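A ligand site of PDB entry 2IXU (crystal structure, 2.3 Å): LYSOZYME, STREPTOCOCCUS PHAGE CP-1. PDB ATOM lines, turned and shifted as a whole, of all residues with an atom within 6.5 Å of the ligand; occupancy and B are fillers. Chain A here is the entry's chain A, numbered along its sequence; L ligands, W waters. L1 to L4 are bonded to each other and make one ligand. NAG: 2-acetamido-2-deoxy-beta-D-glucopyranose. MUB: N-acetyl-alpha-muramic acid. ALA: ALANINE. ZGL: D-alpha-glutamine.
An oxygen (O10) of MUB L2 lies within hydrogen-bond range of the backbone NH (N) of Tyr 153, at 2.9 Å.
The side-chain carboxylate of Glu 94 lies within hydrogen-bond range of an oxygen (O4) of NAG L1, 2.8 Å away.
The backbone carbonyl oxygen of Gly 154 sits at hydrogen-bond distance from a nitrogen (N) of ZGL L4 (2.8 Å).
The side-chain hydroxyl (OH) of Tyr 125 is in hydrogen-bond range of an oxygen (O6) of NAG L1 (3.2 Å).
The backbone carbonyl oxygen (O) of Ser 126 is in hydrogen-bond range of the backbone NH (N) of Ala 151, at 2.9 Å.
The side-chain carboxylate (OD1) of Asp 92 lies close to the side-chain carboxylate (OE2) of Glu 94, at 2.6 Å.
The side-chain hydroxyl (OH) of Tyr 153 sits at hydrogen-bond distance from the side-chain amide oxygen (OE1) of Gln 175 (2.4 Å).
The backbone NH (N) of Gly 152 sits at hydrogen-bond distance from the backbone carbonyl oxygen (O) of Gln 175, at 3.2 Å.
The backbone carbonyl oxygen (O) of Tyr 93 is in hydrogen-bond range of the side-chain hydroxyl (OG) of Ser 126.
The backbone NH (N) of Tyr 93 sits at hydrogen-bond distance from the backbone carbonyl oxygen (O) of Tyr 125 (3.0 Å).
The side-chain hydroxyl of Tyr 125 lies within hydrogen-bond range of the side-chain amide oxygen of Gln 175 (2.6 Å).
C of Ser 126 touches O6 of NAG L1, 3.9 Å away.
CD2 of Tyr 127 touches O6 of NAG L1, 3.2 Å away.
Pro 129 touches the ligand.
Ala 151 touches the ligand.
Gly 152 touches the ligand.
Tyr 164 touches the ligand.
Hydrophobic or aromatic side chains within 4 Å of the ligand: Tyr 125, Tyr 127, Pro 129, Ala 151, Tyr 153 and Tyr 164.
Within 4 Å of the ligand: Glu 94, Tyr 125, Ser 126, Tyr 127, Pro 129, Ala 151, Gly 152, Tyr 153, Gly 154 and Tyr 164.
The nearest printed residue that does not touch the ligand is Leu 155 (4.2 Å).
Water W2 lies within hydrogen-bond range of O of Ala 151 (2.6 Å), O7 of MUB L2 (2.7 Å) and N of Lys 128 (2.9 Å).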
ATOM      1  N   PHE A  61      40.906 -19.965  16.649  1.00  0.00           N
ATOM      2  CA  PHE A  61      39.622 -20.350  17.209  1.00  0.00           C
ATOM      3  C   PHE A  61      39.346 -19.454  18.416  1.00  0.00           C
ATOM      4  O   PHE A  61      40.019 -19.571  19.433  1.00  0.00           O
ATOM      5  CB  PHE A  61      39.601 -21.834  17.610  1.00  0.00           C
ATOM      6  CG  PHE A  61      38.194 -22.362  17.902  1.00  0.00           C
ATOM      7  CD1 PHE A  61      37.432 -22.895  16.894  1.00  0.00           C
ATOM      8  CD2 PHE A  61      37.628 -22.265  19.184  1.00  0.00           C
ATOM      9  CE1 PHE A  61      36.133 -23.357  17.125  1.00  0.00           C
ATOM     10  CE2 PHE A  61      36.319 -22.740  19.448  1.00  0.00           C
ATOM     11  CZ  PHE A  61      35.575 -23.280  18.419  1.00  0.00           C
ATOM     12  N   ASP A  92      37.802 -17.327  13.802  1.00  0.00           N
ATOM     13  CA  ASP A  92      36.837 -18.416  13.851  1.00  0.00           C
ATOM     14  C   ASP A  92      35.980 -18.236  15.093  1.00  0.00           C
ATOM     15  O   ASP A  92      36.450 -18.457  16.217  1.00  0.00           O
ATOM     16  CB  ASP A  92      37.569 -19.775  13.854  1.00  0.00           C
ATOM     17  CG  ASP A  92      36.619 -20.948  13.798  1.00  0.00           C
ATOM     18  OD1 ASP A  92      35.408 -20.831  14.151  1.00  0.00           O
ATOM     19  OD2 ASP A  92      36.971 -22.069  13.369  1.00  0.00           O
ATOM     20  N   TYR A  93      34.745 -17.780  14.903  1.00  0.00           N
ATOM     21  CA  TYR A  93      33.875 -17.373  16.003  1.00  0.00           C
ATOM     22  C   TYR A  93      32.597 -18.188  15.967  1.00  0.00           C
ATOM     23  O   TYR A  93      31.666 -17.900  15.212  1.00  0.00           O
ATOM     24  CB  TYR A  93      33.564 -15.871  15.951  1.00  0.00           C
ATOM     25  CG  TYR A  93      32.925 -15.371  17.244  1.00  0.00           C
ATOM     26  CD1 TYR A  93      33.702 -15.125  18.376  1.00  0.00           C
ATOM     27  CD2 TYR A  93      31.529 -15.144  17.327  1.00  0.00           C
ATOM     28  CE1 TYR A  93      33.102 -14.690  19.580  1.00  0.00           C
ATOM     29  CE2 TYR A  93      30.933 -14.717  18.507  1.00  0.00           C
ATOM     30  CZ  TYR A  93      31.728 -14.502  19.635  1.00  0.00           C
ATOM     31  OH  TYR A  93      31.138 -14.029  20.788  1.00  0.00           O
ATOM     32  N   GLU A  94      32.567 -19.241  16.755  1.00  0.00           N
ATOM     33  CA  GLU A  94      31.532 -20.221  16.583  1.00  0.00           C
ATOM     34  C   GLU A  94      31.196 -20.884  17.871  1.00  0.00           C
ATOM     35  O   GLU A  94      30.349 -21.768  17.892  1.00  0.00           O
ATOM     36  CB  GLU A  94      31.931 -21.240  15.475  1.00  0.00           C
ATOM     37  CG  GLU A  94      33.094 -22.137  15.873  1.00  0.00           C
ATOM     38  CD  GLU A  94      33.296 -23.273  14.890  1.00  0.00           C
ATOM     39  OE1 GLU A  94      32.581 -24.291  14.995  1.00  0.00           O
ATOM     40  OE2 GLU A  94      34.158 -23.095  13.982  1.00  0.00           O
ATOM     41  N   TYR A 125      34.670 -15.914  10.344  1.00  0.00           N
ATOM     42  CA  TYR A 125      34.196 -17.243   9.994  1.00  0.00           C
ATOM     43  C   TYR A 125      33.204 -17.728  10.996  1.00  0.00           C
ATOM     44  O   TYR A 125      33.447 -17.609  12.209  1.00  0.00           O
ATOM     45  CB  TYR A 125      35.354 -18.252   9.959  1.00  0.00           C
ATOM     46  CG  TYR A 125      34.884 -19.669   9.939  1.00  0.00           C
ATOM     47  CD1 TYR A 125      34.543 -20.287   8.732  1.00  0.00           C
ATOM     48  CD2 TYR A 125      34.725 -20.403  11.132  1.00  0.00           C
ATOM     49  CE1 TYR A 125      34.075 -21.618   8.680  1.00  0.00           C
ATOM     50  CE2 TYR A 125      34.256 -21.726  11.085  1.00  0.00           C
ATOM     51  CZ  TYR A 125      33.930 -22.325   9.857  1.00  0.00           C
ATOM     52  OH  TYR A 125      33.465 -23.619   9.806  1.00  0.00           O
ATOM     53  N   SER A 126      32.122 -18.353  10.493  1.00  0.00           N
ATOM     54  CA  SER A 126      31.074 -18.916  11.329  1.00  0.00           C
ATOM     55  C   SER A 126      29.962 -19.587  10.484  1.00  0.00           C
ATOM     56  O   SER A 126      30.124 -19.789   9.255  1.00  0.00           O
ATOM     57  CB  SER A 126      30.458 -17.815  12.213  1.00  0.00           C
ATOM     58  OG  SER A 126      29.799 -18.409  13.335  1.00  0.00           O
ATOM     59  N   TYR A 127      28.848 -19.930  11.136  1.00  0.00           N
ATOM     60  CA  TYR A 127      27.715 -20.423  10.421  1.00  0.00           C
ATOM     61  C   TYR A 127      26.505 -19.517  10.669  1.00  0.00           C
ATOM     62  O   TYR A 127      26.498 -18.758  11.621  1.00  0.00           O
ATOM     63  CB  TYR A 127      27.420 -21.891  10.760  1.00  0.00           C
ATOM     64  CG  TYR A 127      27.143 -22.220  12.208  1.00  0.00           C
ATOM     65  CD1 TYR A 127      25.834 -22.484  12.645  1.00  0.00           C
ATOM     66  CD2 TYR A 127      28.194 -22.349  13.138  1.00  0.00           C
ATOM     67  CE1 TYR A 127      25.552 -22.825  13.970  1.00  0.00           C
ATOM     68  CE2 TYR A 127      27.921 -22.727  14.481  1.00  0.00           C
ATOM     69  CZ  TYR A 127      26.584 -22.952  14.875  1.00  0.00           C
ATOM     70  OH  TYR A 127      26.291 -23.294  16.181  1.00  0.00           O
ATOM     71  N   LYS A 128      25.501 -19.621   9.797  1.00  0.00           N
ATOM     72  CA  LYS A 128      24.392 -18.677   9.780  1.00  0.00           C
ATOM     73  C   LYS A 128      23.566 -18.584  11.082  1.00  0.00           C
ATOM     74  O   LYS A 128      23.556 -17.518  11.680  1.00  0.00           O
ATOM     75  CB  LYS A 128      23.487 -18.899   8.563  1.00  0.00           C
ATOM     76  CG  LYS A 128      22.320 -17.899   8.452  1.00  0.00           C
ATOM     77  CD  LYS A 128      21.608 -18.042   7.110  1.00  0.00           C
ATOM     78  CE  LYS A 128      20.560 -16.897   6.952  1.00  0.00           C
ATOM     79  NZ  LYS A 128      19.756 -17.117   5.725  1.00  0.00           N
ATOM     80  N   PRO A 129      22.870 -19.643  11.525  1.00  0.00           N
ATOM     81  CA  PRO A 129      22.092 -19.520  12.764  1.00  0.00           C
ATOM     82  C   PRO A 129      22.935 -19.012  13.950  1.00  0.00           C
ATOM     83  O   PRO A 129      22.382 -18.216  14.702  1.00  0.00           O
ATOM     84  CB  PRO A 129      21.503 -20.928  12.993  1.00  0.00           C
ATOM     85  CG  PRO A 129      22.302 -21.845  12.094  1.00  0.00           C
ATOM     86  CD  PRO A 129      22.724 -20.989  10.925  1.00  0.00           C
ATOM     87  N   PHE A 130      24.221 -19.368  14.049  1.00  0.00           N
ATOM     88  CA  PHE A 130      25.062 -18.876  15.153  1.00  0.00           C
ATOM     89  C   PHE A 130      25.304 -17.387  15.047  1.00  0.00           C
ATOM     90  O   PHE A 130      25.251 -16.658  16.045  1.00  0.00           O
ATOM     91  CB  PHE A 130      26.422 -19.551  15.162  1.00  0.00           C
ATOM     92  CG  PHE A 130      27.318 -19.128  16.341  1.00  0.00           C
ATOM     93  CD1 PHE A 130      27.322 -19.856  17.553  1.00  0.00           C
ATOM     94  CD2 PHE A 130      28.175 -18.053  16.197  1.00  0.00           C
ATOM     95  CE1 PHE A 130      28.174 -19.499  18.621  1.00  0.00           C
ATOM     96  CE2 PHE A 130      29.028 -17.654  17.224  1.00  0.00           C
ATOM     97  CZ  PHE A 130      29.043 -18.381  18.456  1.00  0.00           C
ATOM     98  N   ALA A 151      29.957 -21.215   6.776  1.00  0.00           N
ATOM     99  CA  ALA A 151      29.739 -22.667   6.666  1.00  0.00           C
ATOM    100  C   ALA A 151      28.246 -22.990   6.497  1.00  0.00           C
ATOM    101  O   ALA A 151      27.419 -22.366   7.136  1.00  0.00           O
ATOM    102  CB  ALA A 151      30.259 -23.352   7.890  1.00  0.00           C
ATOM    103  N   GLY A 152      27.930 -23.953   5.616  1.00  0.00           N
ATOM    104  CA  GLY A 152      26.553 -24.398   5.372  1.00  0.00           C
ATOM    105  C   GLY A 152      26.693 -25.624   4.496  1.00  0.00           C
ATOM    106  O   GLY A 152      27.014 -25.526   3.293  1.00  0.00           O
ATOM    107  N   TYR A 153      26.513 -26.798   5.100  1.00  0.00           N
ATOM    108  CA  TYR A 153      26.882 -28.051   4.478  1.00  0.00           C
ATOM    109  C   TYR A 153      25.746 -28.717   3.707  1.00  0.00           C
ATOM    110  O   TYR A 153      26.000 -29.611   2.904  1.00  0.00           O
ATOM    111  CB  TYR A 153      27.447 -29.022   5.540  1.00  0.00           C
ATOM    112  CG  TYR A 153      28.651 -28.488   6.340  1.00  0.00           C
ATOM    113  CD1 TYR A 153      28.999 -29.053   7.576  1.00  0.00           C
ATOM    114  CD2 TYR A 153      29.452 -27.478   5.839  1.00  0.00           C
ATOM    115  CE1 TYR A 153      30.113 -28.598   8.305  1.00  0.00           C
ATOM    116  CE2 TYR A 153      30.534 -27.015   6.530  1.00  0.00           C
ATOM    117  CZ  TYR A 153      30.869 -27.580   7.763  1.00  0.00           C
ATOM    118  OH  TYR A 153      31.944 -27.080   8.419  1.00  0.00           O
ATOM    119  N   GLY A 154      24.505 -28.306   3.940  1.00  0.00           N
ATOM    120  CA  GLY A 154      23.348 -29.000   3.357  1.00  0.00           C
ATOM    121  C   GLY A 154      23.266 -30.451   3.868  1.00  0.00           C
ATOM    122  O   GLY A 154      23.327 -30.701   5.075  1.00  0.00           O
ATOM    123  N   LEU A 155      23.154 -31.399   2.938  1.00  0.00           N
ATOM    124  CA  LEU A 155      23.205 -32.829   3.233  1.00  0.00           C
ATOM    125  C   LEU A 155      24.604 -33.319   3.634  1.00  0.00           C
ATOM    126  O   LEU A 155      24.736 -34.450   4.109  1.00  0.00           O
ATOM    127  CB  LEU A 155      22.756 -33.639   2.019  1.00  0.00           C
ATOM    128  CG  LEU A 155      21.359 -33.280   1.487  1.00  0.00           C
ATOM    129  CD1 LEU A 155      21.113 -33.820   0.026  1.00  0.00           C
ATOM    130  CD2 LEU A 155      20.321 -33.790   2.477  1.00  0.00           C
ATOM    131  N   ASN A 156      25.609 -32.474   3.416  1.00  0.00           N
ATOM    132  CA  ASN A 156      27.006 -32.713   3.799  1.00  0.00           C
ATOM    133  C   ASN A 156      27.584 -33.972   3.174  1.00  0.00           C
ATOM    134  O   ASN A 156      28.187 -34.800   3.859  1.00  0.00           O
ATOM    135  CB  ASN A 156      27.158 -32.787   5.323  1.00  0.00           C
ATOM    136  CG  ASN A 156      28.569 -32.459   5.790  1.00  0.00           C
ATOM    137  OD1 ASN A 156      28.903 -32.716   6.943  1.00  0.00           O
ATOM    138  ND2 ASN A 156      29.401 -31.890   4.905  1.00  0.00           N
ATOM    139  N   TYR A 164      21.473 -25.311  -0.862  1.00  0.00           N
ATOM    140  CA  TYR A 164      21.688 -25.033   0.555  1.00  0.00           C
ATOM    141  C   TYR A 164      22.642 -23.897   0.785  1.00  0.00           C
ATOM    142  O   TYR A 164      23.053 -23.653   1.924  1.00  0.00           O
ATOM    143  CB  TYR A 164      22.187 -26.283   1.294  1.00  0.00           C
ATOM    144  CG  TYR A 164      21.136 -27.353   1.379  1.00  0.00           C
ATOM    145  CD1 TYR A 164      21.146 -28.420   0.490  1.00  0.00           C
ATOM    146  CD2 TYR A 164      20.147 -27.312   2.363  1.00  0.00           C
ATOM    147  CE1 TYR A 164      20.172 -29.429   0.546  1.00  0.00           C
ATOM    148  CE2 TYR A 164      19.162 -28.318   2.446  1.00  0.00           C
ATOM    149  CZ  TYR A 164      19.173 -29.376   1.546  1.00  0.00           C
ATOM    150  OH  TYR A 164      18.187 -30.382   1.629  1.00  0.00           O
ATOM    151  N   GLN A 175      32.333 -22.563   3.055  1.00  0.00           N
ATOM    152  CA  GLN A 175      32.734 -23.886   3.489  1.00  0.00           C
ATOM    153  C   GLN A 175      31.533 -24.748   3.229  1.00  0.00           C
ATOM    154  O   GLN A 175      30.565 -24.674   3.966  1.00  0.00           O
ATOM    155  CB  GLN A 175      33.094 -23.901   4.971  1.00  0.00           C
ATOM    156  CG  GLN A 175      33.831 -25.148   5.407  1.00  0.00           C
ATOM    157  CD  GLN A 175      34.135 -25.079   6.913  1.00  0.00           C
ATOM    158  OE1 GLN A 175      33.219 -25.110   7.724  1.00  0.00           O
ATOM    159  NE2 GLN A 175      35.395 -24.868   7.260  1.00  0.00           N
ATOM    160  N   ASP A 182      37.319 -30.524   5.699  1.00  0.00           N
ATOM    161  CA  ASP A 182      36.711 -29.211   5.379  1.00  0.00           C
ATOM    162  C   ASP A 182      36.981 -28.735   3.968  1.00  0.00           C
ATOM    163  O   ASP A 182      38.129 -28.542   3.567  1.00  0.00           O
ATOM    164  CB  ASP A 182      37.214 -28.110   6.309  1.00  0.00           C
ATOM    165  CG  ASP A 182      36.615 -28.186   7.717  1.00  0.00           C
ATOM    166  OD1 ASP A 182      35.738 -29.033   7.939  1.00  0.00           O
ATOM    167  OD2 ASP A 182      36.978 -27.448   8.645  1.00  0.00           O
HETATM  168  C1  NAG L   1      28.476 -26.816  13.250  1.00  0.00           C
HETATM  169  C2  NAG L   1      29.467 -27.984  13.423  1.00  0.00           C
HETATM  170  C3  NAG L   1      30.850 -27.402  13.671  1.00  0.00           C
HETATM  171  C4  NAG L   1      31.248 -26.528  12.506  1.00  0.00           C
HETATM  172  C5  NAG L   1      30.236 -25.400  12.364  1.00  0.00           C
HETATM  173  C6  NAG L   1      30.510 -24.457  11.208  1.00  0.00           C
HETATM  174  C7  NAG L   1      28.190 -29.744  14.519  1.00  0.00           C
HETATM  175  C8  NAG L   1      27.827 -30.435  15.821  1.00  0.00           C
HETATM  176  N2  NAG L   1      29.095 -28.769  14.594  1.00  0.00           N
HETATM  177  O3  NAG L   1      31.785 -28.465  13.805  1.00  0.00           O
HETATM  178  O4  NAG L   1      32.544 -25.993  12.742  1.00  0.00           O
HETATM  179  O5  NAG L   1      28.888 -25.970  12.162  1.00  0.00           O
HETATM  180  O6  NAG L   1      30.881 -23.169  11.672  1.00  0.00           O
HETATM  181  O7  NAG L   1      27.657 -30.088  13.468  1.00  0.00           O
HETATM  182  C1  MUB L   2      23.181 -26.172  13.040  1.00  0.00           C
HETATM  183  C2  MUB L   2      24.037 -25.631  11.871  1.00  0.00           C
HETATM  184  C3  MUB L   2      25.295 -26.505  11.729  1.00  0.00           C
HETATM  185  C4  MUB L   2      26.070 -26.510  13.035  1.00  0.00           C
HETATM  186  C5  MUB L   2      25.176 -27.047  14.152  1.00  0.00           C
HETATM  187  C6  MUB L   2      25.900 -27.034  15.505  1.00  0.00           C
HETATM  188  C7  MUB L   2      23.267 -24.600   9.774  1.00  0.00           C
HETATM  189  C8  MUB L   2      22.375 -24.718   8.538  1.00  0.00           C
HETATM  190  C9  MUB L   2      26.791 -26.728   9.599  1.00  0.00           C
HETATM  191  C10 MUB L   2      25.793 -27.221   8.609  1.00  0.00           C
HETATM  192  C11 MUB L   2      27.963 -25.936   9.016  1.00  0.00           C
HETATM  193  O1  MUB L   2      22.736 -27.494  12.741  1.00  0.00           O
HETATM  194  O3  MUB L   2      26.115 -26.001  10.654  1.00  0.00           O
HETATM  195  O4  MUB L   2      27.235 -27.337  12.905  1.00  0.00           O
HETATM  196  O5  MUB L   2      23.963 -26.213  14.259  1.00  0.00           O
HETATM  197  O6  MUB L   2      24.982 -27.240  16.591  1.00  0.00           O
HETATM  198  O7  MUB L   2      23.983 -23.608   9.913  1.00  0.00           O
HETATM  199  O10 MUB L   2      25.324 -26.492   7.735  1.00  0.00           O
HETATM  200  N2  MUB L   2      23.237 -25.612  10.644  1.00  0.00           N
HETATM  201  N   ALA L   3      25.483 -28.517   8.811  1.00  0.00           N
HETATM  202  CA  ALA L   3      24.536 -29.285   7.990  1.00  0.00           C
HETATM  203  C   ALA L   3      23.080 -28.881   8.226  1.00  0.00           C
HETATM  204  O   ALA L   3      22.750 -28.314   9.286  1.00  0.00           O
HETATM  205  CB  ALA L   3      24.696 -30.777   8.263  1.00  0.00           C
HETATM  206  CD  ZGL L   4      20.302 -27.715   6.877  1.00  0.00           C
HETATM  207  N   ZGL L   4      22.225 -29.261   7.256  1.00  0.00           N
HETATM  208  O2  ZGL L   4      21.034 -27.063   6.092  1.00  0.00           O
HETATM  209  N1  ZGL L   4      19.192 -27.328   7.284  1.00  0.00           N
HETATM  210  CA  ZGL L   4      20.787 -29.067   7.409  1.00  0.00           C
HETATM  211  CB  ZGL L   4      19.993 -30.194   6.762  1.00  0.00           C
HETATM  212  C   ZGL L   4      19.527 -32.681   6.924  1.00  0.00           C
HETATM  213  CG  ZGL L   4      20.255 -31.495   7.488  1.00  0.00           C
HETATM  214  OXT ZGL L   4      18.281 -32.616   6.754  1.00  0.00           O
HETATM  215  O   ZGL L   4      20.218 -33.684   6.668  1.00  0.00           O
HETATM  216  O   HOH W   1      34.346 -28.529  13.212  1.00  0.00           O
HETATM  217  O   HOH W   2      25.000 -21.841   8.081  1.00  0.00           O
HETATM  218  O   HOH W   3      26.665 -29.916  11.132  1.00  0.00           O
